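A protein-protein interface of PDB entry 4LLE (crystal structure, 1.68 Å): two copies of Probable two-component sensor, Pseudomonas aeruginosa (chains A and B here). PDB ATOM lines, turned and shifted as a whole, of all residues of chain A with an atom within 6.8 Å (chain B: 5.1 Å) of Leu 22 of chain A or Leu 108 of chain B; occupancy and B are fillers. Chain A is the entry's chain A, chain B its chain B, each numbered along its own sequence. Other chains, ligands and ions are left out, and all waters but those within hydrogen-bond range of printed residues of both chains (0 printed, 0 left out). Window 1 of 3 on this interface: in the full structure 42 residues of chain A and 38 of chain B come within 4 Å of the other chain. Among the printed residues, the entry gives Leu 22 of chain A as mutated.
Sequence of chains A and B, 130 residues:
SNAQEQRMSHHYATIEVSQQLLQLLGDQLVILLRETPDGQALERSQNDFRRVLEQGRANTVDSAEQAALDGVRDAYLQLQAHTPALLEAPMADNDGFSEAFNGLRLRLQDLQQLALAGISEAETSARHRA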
ATOM      1  N   VAL A  17      32.809  13.371  15.813  1.00  0.00           N
ATOM      2  CA  VAL A  17      32.454  14.724  15.362  1.00  0.00           C
ATOM      3  C   VAL A  17      31.339  15.307  16.241  1.00  0.00           C
ATOM      4  O   VAL A  17      31.423  16.455  16.692  1.00  0.00           O
ATOM      5  CB  VAL A  17      32.028  14.747  13.889  1.00  0.00           C
ATOM      6  CG1 VAL A  17      31.414  16.112  13.516  1.00  0.00           C
ATOM      7  CG2 VAL A  17      33.221  14.448  13.008  1.00  0.00           C
ATOM      8  N   SER A  18      30.309  14.513  16.501  1.00  0.00           N
ATOM      9  CA  SER A  18      29.196  14.995  17.321  1.00  0.00           C
ATOM     10  C   SER A  18      29.650  15.334  18.737  1.00  0.00           C
ATOM     11  O   SER A  18      29.176  16.296  19.309  1.00  0.00           O
ATOM     12  CB  SER A  18      28.049  13.979  17.337  1.00  0.00           C
ATOM     13  OG  SER A  18      28.337  12.906  18.219  1.00  0.00           O
ATOM     14  N   GLN A  19      30.591  14.563  19.284  1.00  0.00           N
ATOM     15  CA  GLN A  19      31.105  14.828  20.623  1.00  0.00           C
ATOM     16  C   GLN A  19      31.891  16.134  20.670  1.00  0.00           C
ATOM     17  O   GLN A  19      31.744  16.926  21.600  1.00  0.00           O
ATOM     18  CB  GLN A  19      31.971  13.663  21.109  1.00  0.00           C
ATOM     19  CG  GLN A  19      31.177  12.539  21.767  1.00  0.00           C
ATOM     20  CD  GLN A  19      30.515  12.980  23.064  1.00  0.00           C
ATOM     21  OE1 GLN A  19      31.182  13.430  23.995  1.00  0.00           O
ATOM     22  NE2 GLN A  19      29.196  12.857  23.127  1.00  0.00           N
ATOM     23  N   GLN A  20      32.719  16.353  19.658  1.00  0.00           N
ATOM     24  CA  GLN A  20      33.506  17.577  19.588  1.00  0.00           C
ATOM     25  C   GLN A  20      32.579  18.789  19.456  1.00  0.00           C
ATOM     26  O   GLN A  20      32.814  19.827  20.086  1.00  0.00           O
ATOM     27  CB  GLN A  20      34.515  17.512  18.444  1.00  0.00           C
ATOM     28  CG  GLN A  20      35.488  18.670  18.438  1.00  0.00           C
ATOM     29  CD  GLN A  20      36.720  18.411  17.581  1.00  0.00           C
ATOM     30  OE1 GLN A  20      36.746  17.489  16.759  1.00  0.00           O
ATOM     31  NE2 GLN A  20      37.752  19.225  17.780  1.00  0.00           N
ATOM     32  N   LEU A  21      31.530  18.670  18.643  1.00  0.00           N
ATOM     33  CA  LEU A  21      30.593  19.794  18.490  1.00  0.00           C
ATOM     34  C   LEU A  21      29.826  20.066  19.775  1.00  0.00           C
ATOM     35  O   LEU A  21      29.609  21.208  20.153  1.00  0.00           O
ATOM     36  CB  LEU A  21      29.622  19.587  17.314  1.00  0.00           C
ATOM     37  CG  LEU A  21      30.305  19.541  15.949  1.00  0.00           C
ATOM     38  CD1 LEU A  21      29.265  19.251  14.868  1.00  0.00           C
ATOM     39  CD2 LEU A  21      31.081  20.850  15.661  1.00  0.00           C
ATOM     40  N   LEU A  22      29.412  19.010  20.465  1.00  0.00           N
ATOM     41  CA  LEU A  22      28.676  19.212  21.713  1.00  0.00           C
ATOM     42  C   LEU A  22      29.577  19.870  22.737  1.00  0.00           C
ATOM     43  O   LEU A  22      29.142  20.713  23.515  1.00  0.00           O
ATOM     44  CB  LEU A  22      28.171  17.876  22.251  1.00  0.00           C
ATOM     45  CG  LEU A  22      26.907  17.420  21.516  1.00  0.00           C
ATOM     46  CD1 LEU A  22      26.629  15.962  21.797  1.00  0.00           C
ATOM     47  CD2 LEU A  22      25.715  18.291  21.948  1.00  0.00           C
ATOM     48  N   GLN A  23      30.852  19.504  22.707  1.00  0.00           N
ATOM     49  CA  GLN A  23      31.827  20.090  23.614  1.00  0.00           C
ATOM     50  C   GLN A  23      31.975  21.585  23.340  1.00  0.00           C
ATOM     51  O   GLN A  23      31.972  22.386  24.262  1.00  0.00           O
ATOM     52  CB  GLN A  23      33.166  19.372  23.477  1.00  0.00           C
ATOM     53  CG  GLN A  23      34.323  20.038  24.184  1.00  0.00           C
ATOM     54  CD  GLN A  23      35.572  19.174  24.174  1.00  0.00           C
ATOM     55  OE1 GLN A  23      36.689  19.678  24.053  1.00  0.00           O
ATOM     56  NE2 GLN A  23      35.386  17.864  24.301  1.00  0.00           N
ATOM     57  N   LEU A  24      32.090  21.942  22.064  1.00  0.00           N
ATOM     58  CA  LEU A  24      32.246  23.347  21.676  1.00  0.00           C
ATOM     59  C   LEU A  24      30.975  24.129  21.989  1.00  0.00           C
ATOM     60  O   LEU A  24      31.027  25.289  22.395  1.00  0.00           O
ATOM     61  CB  LEU A  24      32.611  23.460  20.197  1.00  0.00           C
ATOM     62  CG  LEU A  24      34.050  23.029  19.907  1.00  0.00           C
ATOM     63  CD1 LEU A  24      34.311  22.873  18.410  1.00  0.00           C
ATOM     64  CD2 LEU A  24      35.008  24.046  20.505  1.00  0.00           C
ATOM     65  N   LEU A  25      29.824  23.489  21.810  1.00  0.00           N
ATOM     66  CA  LEU A  25      28.587  24.158  22.157  1.00  0.00           C
ATOM     67  C   LEU A  25      28.554  24.446  23.656  1.00  0.00           C
ATOM     68  O   LEU A  25      28.183  25.548  24.070  1.00  0.00           O
ATOM     69  CB  LEU A  25      27.377  23.314  21.729  1.00  0.00           C
ATOM     70  CG  LEU A  25      26.002  23.926  22.009  1.00  0.00           C
ATOM     71  CD1 LEU A  25      25.767  25.324  21.385  1.00  0.00           C
ATOM     72  CD2 LEU A  25      24.940  22.960  21.494  1.00  0.00           C
ATOM     73  N   GLY A  26      28.946  23.468  24.470  1.00  0.00           N
ATOM     74  CA  GLY A  26      29.050  23.681  25.904  1.00  0.00           C
ATOM     75  C   GLY A  26      29.993  24.832  26.235  1.00  0.00           C
ATOM     76  O   GLY A  26      29.698  25.665  27.095  1.00  0.00           O
ATOM     77  N   ASP A  27      31.121  24.871  25.535  1.00  0.00           N
ATOM     78  CA  ASP A  27      32.119  25.921  25.742  1.00  0.00           C
ATOM     79  C   ASP A  27      31.452  27.268  25.527  1.00  0.00           C
ATOM     80  O   ASP A  27      31.710  28.208  26.261  1.00  0.00           O
ATOM     81  CB  ASP A  27      33.270  25.822  24.732  1.00  0.00           C
ATOM     82  CG  ASP A  27      34.139  24.604  24.921  1.00  0.00           C
ATOM     83  OD1 ASP A  27      34.100  23.987  26.004  1.00  0.00           O
ATOM     84  OD2 ASP A  27      34.907  24.282  23.973  1.00  0.00           O
ATOM     85  N   LEU A  29      28.234  27.985  25.783  1.00  0.00           N
ATOM     86  CA  LEU A  29      27.312  28.231  26.880  1.00  0.00           C
ATOM     87  C   LEU A  29      28.064  28.684  28.131  1.00  0.00           C
ATOM     88  O   LEU A  29      27.621  29.591  28.827  1.00  0.00           O
ATOM     89  CB  LEU A  29      26.514  26.971  27.193  1.00  0.00           C
ATOM     90  CG  LEU A  29      25.511  26.497  26.148  1.00  0.00           C
ATOM     91  CD1 LEU A  29      25.021  25.106  26.527  1.00  0.00           C
ATOM     92  CD2 LEU A  29      24.362  27.475  26.019  1.00  0.00           C
ATOM     93  N   PHE A  49      33.775  25.830  16.212  1.00  0.00           N
ATOM     94  CA  PHE A  49      32.606  25.007  15.889  1.00  0.00           C
ATOM     95  C   PHE A  49      32.400  24.941  14.371  1.00  0.00           C
ATOM     96  O   PHE A  49      32.256  23.867  13.796  1.00  0.00           O
ATOM     97  CB  PHE A  49      31.359  25.530  16.631  1.00  0.00           C
ATOM     98  CG  PHE A  49      30.144  24.637  16.516  1.00  0.00           C
ATOM     99  CD1 PHE A  49      29.445  24.525  15.316  1.00  0.00           C
ATOM    100  CD2 PHE A  49      29.699  23.926  17.624  1.00  0.00           C
ATOM    101  CE1 PHE A  49      28.318  23.695  15.217  1.00  0.00           C
ATOM    102  CE2 PHE A  49      28.568  23.109  17.539  1.00  0.00           C
ATOM    103  CZ  PHE A  49      27.889  22.992  16.332  1.00  0.00           C
ATOM    104  N   LEU A  53      32.663  21.472  12.246  1.00  0.00           N
ATOM    105  CA  LEU A  53      31.438  21.065  11.551  1.00  0.00           C
ATOM    106  C   LEU A  53      31.707  20.894  10.065  1.00  0.00           C
ATOM    107  O   LEU A  53      31.257  19.928   9.447  1.00  0.00           O
ATOM    108  CB  LEU A  53      30.319  22.089  11.741  1.00  0.00           C
ATOM    109  CG  LEU A  53      29.064  21.866  10.885  1.00  0.00           C
ATOM    110  CD1 LEU A  53      28.490  20.501  11.137  1.00  0.00           C
ATOM    111  CD2 LEU A  53      28.045  22.960  11.194  1.00  0.00           C
ATOM    112  N   LEU A  69      24.162  16.166   9.476  1.00  0.00           N
ATOM    113  CA  LEU A  69      25.117  17.257   9.685  1.00  0.00           C
ATOM    114  C   LEU A  69      24.724  18.534   8.943  1.00  0.00           C
ATOM    115  O   LEU A  69      25.067  19.632   9.362  1.00  0.00           O
ATOM    116  CB  LEU A  69      26.533  16.832   9.277  1.00  0.00           C
ATOM    117  CG  LEU A  69      27.222  16.001  10.359  1.00  0.00           C
ATOM    118  CD1 LEU A  69      28.436  15.275   9.820  1.00  0.00           C
ATOM    119  CD2 LEU A  69      27.570  16.872  11.588  1.00  0.00           C
ATOM    120  N   VAL A  72      22.475  20.091  11.267  1.00  0.00           N
ATOM    121  CA  VAL A  72      23.268  20.730  12.322  1.00  0.00           C
ATOM    122  C   VAL A  72      23.773  22.095  11.876  1.00  0.00           C
ATOM    123  O   VAL A  72      23.728  23.056  12.631  1.00  0.00           O
ATOM    124  CB  VAL A  72      24.437  19.848  12.749  1.00  0.00           C
ATOM    125  CG1 VAL A  72      25.361  20.622  13.694  1.00  0.00           C
ATOM    126  CG2 VAL A  72      23.893  18.622  13.468  1.00  0.00           C
ATOM    127  N   ARG A 105      29.062  19.064  33.042  1.00  0.00           N
ATOM    128  CA  ARG A 105      28.975  18.593  31.664  1.00  0.00           C
ATOM    129  C   ARG A 105      30.222  17.823  31.223  1.00  0.00           C
ATOM    130  O   ARG A 105      30.118  16.887  30.449  1.00  0.00           O
ATOM    131  CB  ARG A 105      28.590  19.723  30.698  1.00  0.00           C
ATOM    132  CG  ARG A 105      29.593  20.884  30.627  1.00  0.00           C
ATOM    133  CD  ARG A 105      30.428  20.774  29.372  1.00  0.00           C
ATOM    134  NE  ARG A 105      31.427  21.839  29.299  1.00  0.00           N
ATOM    135  CZ  ARG A 105      32.016  22.217  28.170  1.00  0.00           C
ATOM    136  NH1 ARG A 105      32.925  23.183  28.185  1.00  0.00           N
ATOM    137  NH2 ARG A 105      31.695  21.627  27.029  1.00  0.00           N
ATOM    138  N   GLN A 109      30.252  14.023  29.777  1.00  0.00           N
ATOM    139  CA  GLN A 109      30.794  13.778  28.442  1.00  0.00           C
ATOM    140  C   GLN A 109      31.933  12.779  28.512  1.00  0.00           C
ATOM    141  O   GLN A 109      32.071  11.904  27.657  1.00  0.00           O
ATOM    142  CB  GLN A 109      31.269  15.092  27.795  1.00  0.00           C
ATOM    143  CG  GLN A 109      30.143  16.110  27.581  1.00  0.00           C
ATOM    144  CD  GLN A 109      30.469  17.153  26.523  1.00  0.00           C
ATOM    145  OE1 GLN A 109      30.822  18.292  26.840  1.00  0.00           O
ATOM    146  NE2 GLN A 109      30.339  16.768  25.255  1.00  0.00           N
ATOM    147  N   GLN A 112      30.592   9.213  29.066  1.00  0.00           N
ATOM    148  CA  GLN A 112      30.037   8.750  27.809  1.00  0.00           C
ATOM    149  C   GLN A 112      31.150   8.218  26.914  1.00  0.00           C
ATOM    150  O   GLN A 112      31.053   7.118  26.379  1.00  0.00           O
ATOM    151  CB  GLN A 112      29.327   9.907  27.131  1.00  0.00           C
ATOM    152  CG  GLN A 112      28.379   9.533  26.024  1.00  0.00           C
ATOM    153  CD  GLN A 112      27.446  10.680  25.703  1.00  0.00           C
ATOM    154  OE1 GLN A 112      27.530  11.286  24.639  1.00  0.00           O
ATOM    155  NE2 GLN A 112      26.560  10.996  26.637  1.00  0.00           N
ATOM    156  N   LEU B 104      19.529  22.897  18.133  1.00  0.00           N
ATOM    157  CA  LEU B 104      20.871  22.454  17.791  1.00  0.00           C
ATOM    158  C   LEU B 104      21.270  21.277  18.679  1.00  0.00           C
ATOM    159  O   LEU B 104      21.798  20.268  18.199  1.00  0.00           O
ATOM    160  CB  LEU B 104      21.847  23.622  17.974  1.00  0.00           C
ATOM    161  CG  LEU B 104      23.312  23.236  17.765  1.00  0.00           C
ATOM    162  CD1 LEU B 104      23.509  22.716  16.341  1.00  0.00           C
ATOM    163  CD2 LEU B 104      24.213  24.461  18.031  1.00  0.00           C
ATOM    164  N   ARG B 105      21.020  21.387  19.984  1.00  0.00           N
ATOM    165  CA  ARG B 105      21.517  20.333  20.882  1.00  0.00           C
ATOM    166  C   ARG B 105      20.748  19.037  20.634  1.00  0.00           C
ATOM    167  O   ARG B 105      21.311  17.950  20.710  1.00  0.00           O
ATOM    168  CB  ARG B 105      21.512  20.770  22.357  1.00  0.00           C
ATOM    169  CG  ARG B 105      20.139  21.037  22.932  1.00  0.00           C
ATOM    170  CD  ARG B 105      19.604  19.815  23.651  1.00  0.00           C
ATOM    171  NE  ARG B 105      18.272  20.102  24.171  1.00  0.00           N
ATOM    172  CZ  ARG B 105      17.757  19.536  25.253  1.00  0.00           C
ATOM    173  NH1 ARG B 105      16.527  19.860  25.640  1.00  0.00           N
ATOM    174  NH2 ARG B 105      18.467  18.650  25.938  1.00  0.00           N
ATOM    175  N   LEU B 106      19.468  19.138  20.281  1.00  0.00           N
ATOM    176  CA  LEU B 106      18.723  17.930  19.936  1.00  0.00           C
ATOM    177  C   LEU B 106      19.265  17.252  18.696  1.00  0.00           C
ATOM    178  O   LEU B 106      19.379  16.038  18.642  1.00  0.00           O
ATOM    179  CB  LEU B 106      17.243  18.236  19.735  1.00  0.00           C
ATOM    180  CG  LEU B 106      16.549  18.622  21.031  1.00  0.00           C
ATOM    181  CD1 LEU B 106      15.143  19.069  20.673  1.00  0.00           C
ATOM    182  CD2 LEU B 106      16.514  17.484  22.040  1.00  0.00           C
ATOM    183  N   ARG B 107      19.579  18.045  17.676  1.00  0.00           N
ATOM    184  CA  ARG B 107      20.144  17.490  16.452  1.00  0.00           C
ATOM    185  C   ARG B 107      21.496  16.795  16.676  1.00  0.00           C
ATOM    186  O   ARG B 107      21.769  15.737  16.095  1.00  0.00           O
ATOM    187  CB  ARG B 107      20.311  18.595  15.415  1.00  0.00           C
ATOM    188  CG  ARG B 107      19.004  19.009  14.754  1.00  0.00           C
ATOM    189  CD  ARG B 107      19.243  20.073  13.708  1.00  0.00           C
ATOM    190  NE  ARG B 107      17.977  20.624  13.233  1.00  0.00           N
ATOM    191  CZ  ARG B 107      17.193  20.028  12.341  1.00  0.00           C
ATOM    192  NH1 ARG B 107      17.546  18.867  11.803  1.00  0.00           N
ATOM    193  NH2 ARG B 107      16.046  20.598  11.988  1.00  0.00           N
ATOM    194  N   LEU B 108      22.337  17.409  17.493  1.00  0.00           N
ATOM    195  CA  LEU B 108      23.620  16.798  17.825  1.00  0.00           C
ATOM    196  C   LEU B 108      23.424  15.505  18.596  1.00  0.00           C
ATOM    197  O   LEU B 108      24.059  14.509  18.288  1.00  0.00           O
ATOM    198  CB  LEU B 108      24.484  17.756  18.633  1.00  0.00           C
ATOM    199  CG  LEU B 108      25.039  18.878  17.766  1.00  0.00           C
ATOM    200  CD1 LEU B 108      25.701  19.945  18.639  1.00  0.00           C
ATOM    201  CD2 LEU B 108      26.036  18.324  16.757  1.00  0.00           C
ATOM    202  N   GLN B 109      22.539  15.529  19.592  1.00  0.00           N
ATOM    203  CA  GLN B 109      22.263  14.335  20.405  1.00  0.00           C
ATOM    204  C   GLN B 109      21.719  13.250  19.507  1.00  0.00           C
ATOM    205  O   GLN B 109      22.107  12.084  19.589  1.00  0.00           O
ATOM    206  CB  GLN B 109      21.247  14.673  21.490  1.00  0.00           C
ATOM    207  CG  GLN B 109      20.300  13.532  21.841  1.00  0.00           C
ATOM    208  CD  GLN B 109      19.010  14.025  22.477  1.00  0.00           C
ATOM    209  OE1 GLN B 109      18.981  15.074  23.120  1.00  0.00           O
ATOM    210  NE2 GLN B 109      17.934  13.277  22.286  1.00  0.00           N
ATOM    211  N   ASP B 110      20.813  13.634  18.621  1.00  0.00           N
ATOM    212  CA  ASP B 110      20.181  12.635  17.778  1.00  0.00           C
ATOM    213  C   ASP B 110      21.161  12.033  16.776  1.00  0.00           C
ATOM    214  O   ASP B 110      21.089  10.844  16.485  1.00  0.00           O
ATOM    215  CB  ASP B 110      18.941  13.207  17.085  1.00  0.00           C
ATOM    216  CG  ASP B 110      17.842  13.558  18.076  1.00  0.00           C
ATOM    217  OD1 ASP B 110      17.958  13.173  19.264  1.00  0.00           O
ATOM    218  OD2 ASP B 110      16.862  14.219  17.671  1.00  0.00           O
ATOM    219  N   LEU B 111      22.087  12.856  16.275  1.00  0.00           N
ATOM    220  CA  LEU B 111      23.097  12.398  15.329  1.00  0.00           C
ATOM    221  C   LEU B 111      23.996  11.376  16.009  1.00  0.00           C
ATOM    222  O   LEU B 111      24.350  10.343  15.431  1.00  0.00           O
ATOM    223  CB  LEU B 111      23.937  13.569  14.830  1.00  0.00           C
ATOM    224  CG  LEU B 111      25.234  13.223  14.099  1.00  0.00           C
ATOM    225  CD1 LEU B 111      24.949  12.457  12.812  1.00  0.00           C
ATOM    226  CD2 LEU B 111      26.041  14.494  13.818  1.00  0.00           C
ATOM    227  N   GLN B 112      24.366  11.662  17.249  1.00  0.00           N
ATOM    228  CA  GLN B 112      25.225  10.743  17.981  1.00  0.00           C
ATOM    229  C   GLN B 112      24.521   9.396  18.131  1.00  0.00           C
ATOM    230  O   GLN B 112      25.123   8.338  17.965  1.00  0.00           O
ATOM    231  CB  GLN B 112      25.535  11.320  19.350  1.00  0.00           C
ATOM    232  CG  GLN B 112      26.604  10.580  20.100  1.00  0.00           C
ATOM    233  CD  GLN B 112      27.245  11.467  21.130  1.00  0.00           C
ATOM    234  OE1 GLN B 112      28.324  12.011  20.906  1.00  0.00           O
ATOM    235  NE2 GLN B 112      26.567  11.649  22.255  1.00  0.00           N
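OG of Ser 18 of chain A lies within hydrogen-bond range of OE1 of Gln 112 of chain B (2.8 Å). OE1 of Gln 112 of chain A lies within hydrogen-bond range of NE2 of Gln 112 of chain B. The side-chain amide oxygen (OE1) of Gln 112 of chain B lies within hydrogen-bond range of the side-chain amide nitrogen (NE2) of Gln 19 of chain A (2.5 Å).
Gln 112 of chain B touches its own counterpart, Gln 112 of chain A. Positions printed for both chains: 105, 109 and 112. Of the 9 pairs that touch across the chains among the printed residues, 1 has its exchanged pair printed and touching as well.
Among the printed residues, merely in contact across the chains: Leu 22 of chain A with Leu 108 of chain B (3.6 Å), Leu 69 of chain A with Leu 111 of chain B (3.6 Å), Val 72 of chain A with Leu 104 of chain B (3.7 Å), Leu 25 of chain A with Leu 104 of chain B (3.8 Å), Leu 21 of chain A with Leu 108 of chain B (3.8 Å) and Val 72 of chain A with Leu 108 of chain B (3.9 Å).
Along chain B the printed residues that touch a printed residue of chain A span positions 104 to 112. Printed residues of chain A that touch a printed residue of chain B: Ser 18, Gln 19, Leu 21, Leu 22, Leu 25, Leu 69, Val 72 and Gln 112. Hydrophobic or aromatic side chains of chain A that line the printed part of chain B: Leu 21, Leu 22, Leu 25, Leu 69 and Val 72. Among the printed residues, no Asp or Glu carboxylate lies within 4 Å of a Lys or Arg side-chain nitrogen of the other chain.
The side-chain amide nitrogen (NE2) of Gln 19 of chain A is in hydrogen-bond range of the side-chain amide oxygen (OE1) of Gln 112 of chain A, at 2.7 Å.
Of chain B, only Leu 108 comes within 4 Å of Leu 22 of chain A. Of chain A, only Leu 21 (3.8 Å), Leu 22 (3.6 Å) and Val 72 (3.9 Å) come within 4 Å of Leu 108 of chain B. Printed residues of chain B within 4 Å of Val 72 of chain A: Leu 104 (3.7 Å) and Leu 108 (3.9 Å). Of the printed residues of chain B, Leu 21 of chain A touches Leu 108. Of the printed residues of chain A, Gln 112 of chain B touches Ser 18 (2.8 Å), Gln 19 (2.5 Å) and Gln 112 (2.6 Å). Arg 105 of chain A touches none of the printed residues of chain B. Leu 106 of chain B touches none of the printed residues of chain A. The nearest residue of chain B that does not touch Leu 22 of chain A is Gln 112 of chain B (4.3 Å).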
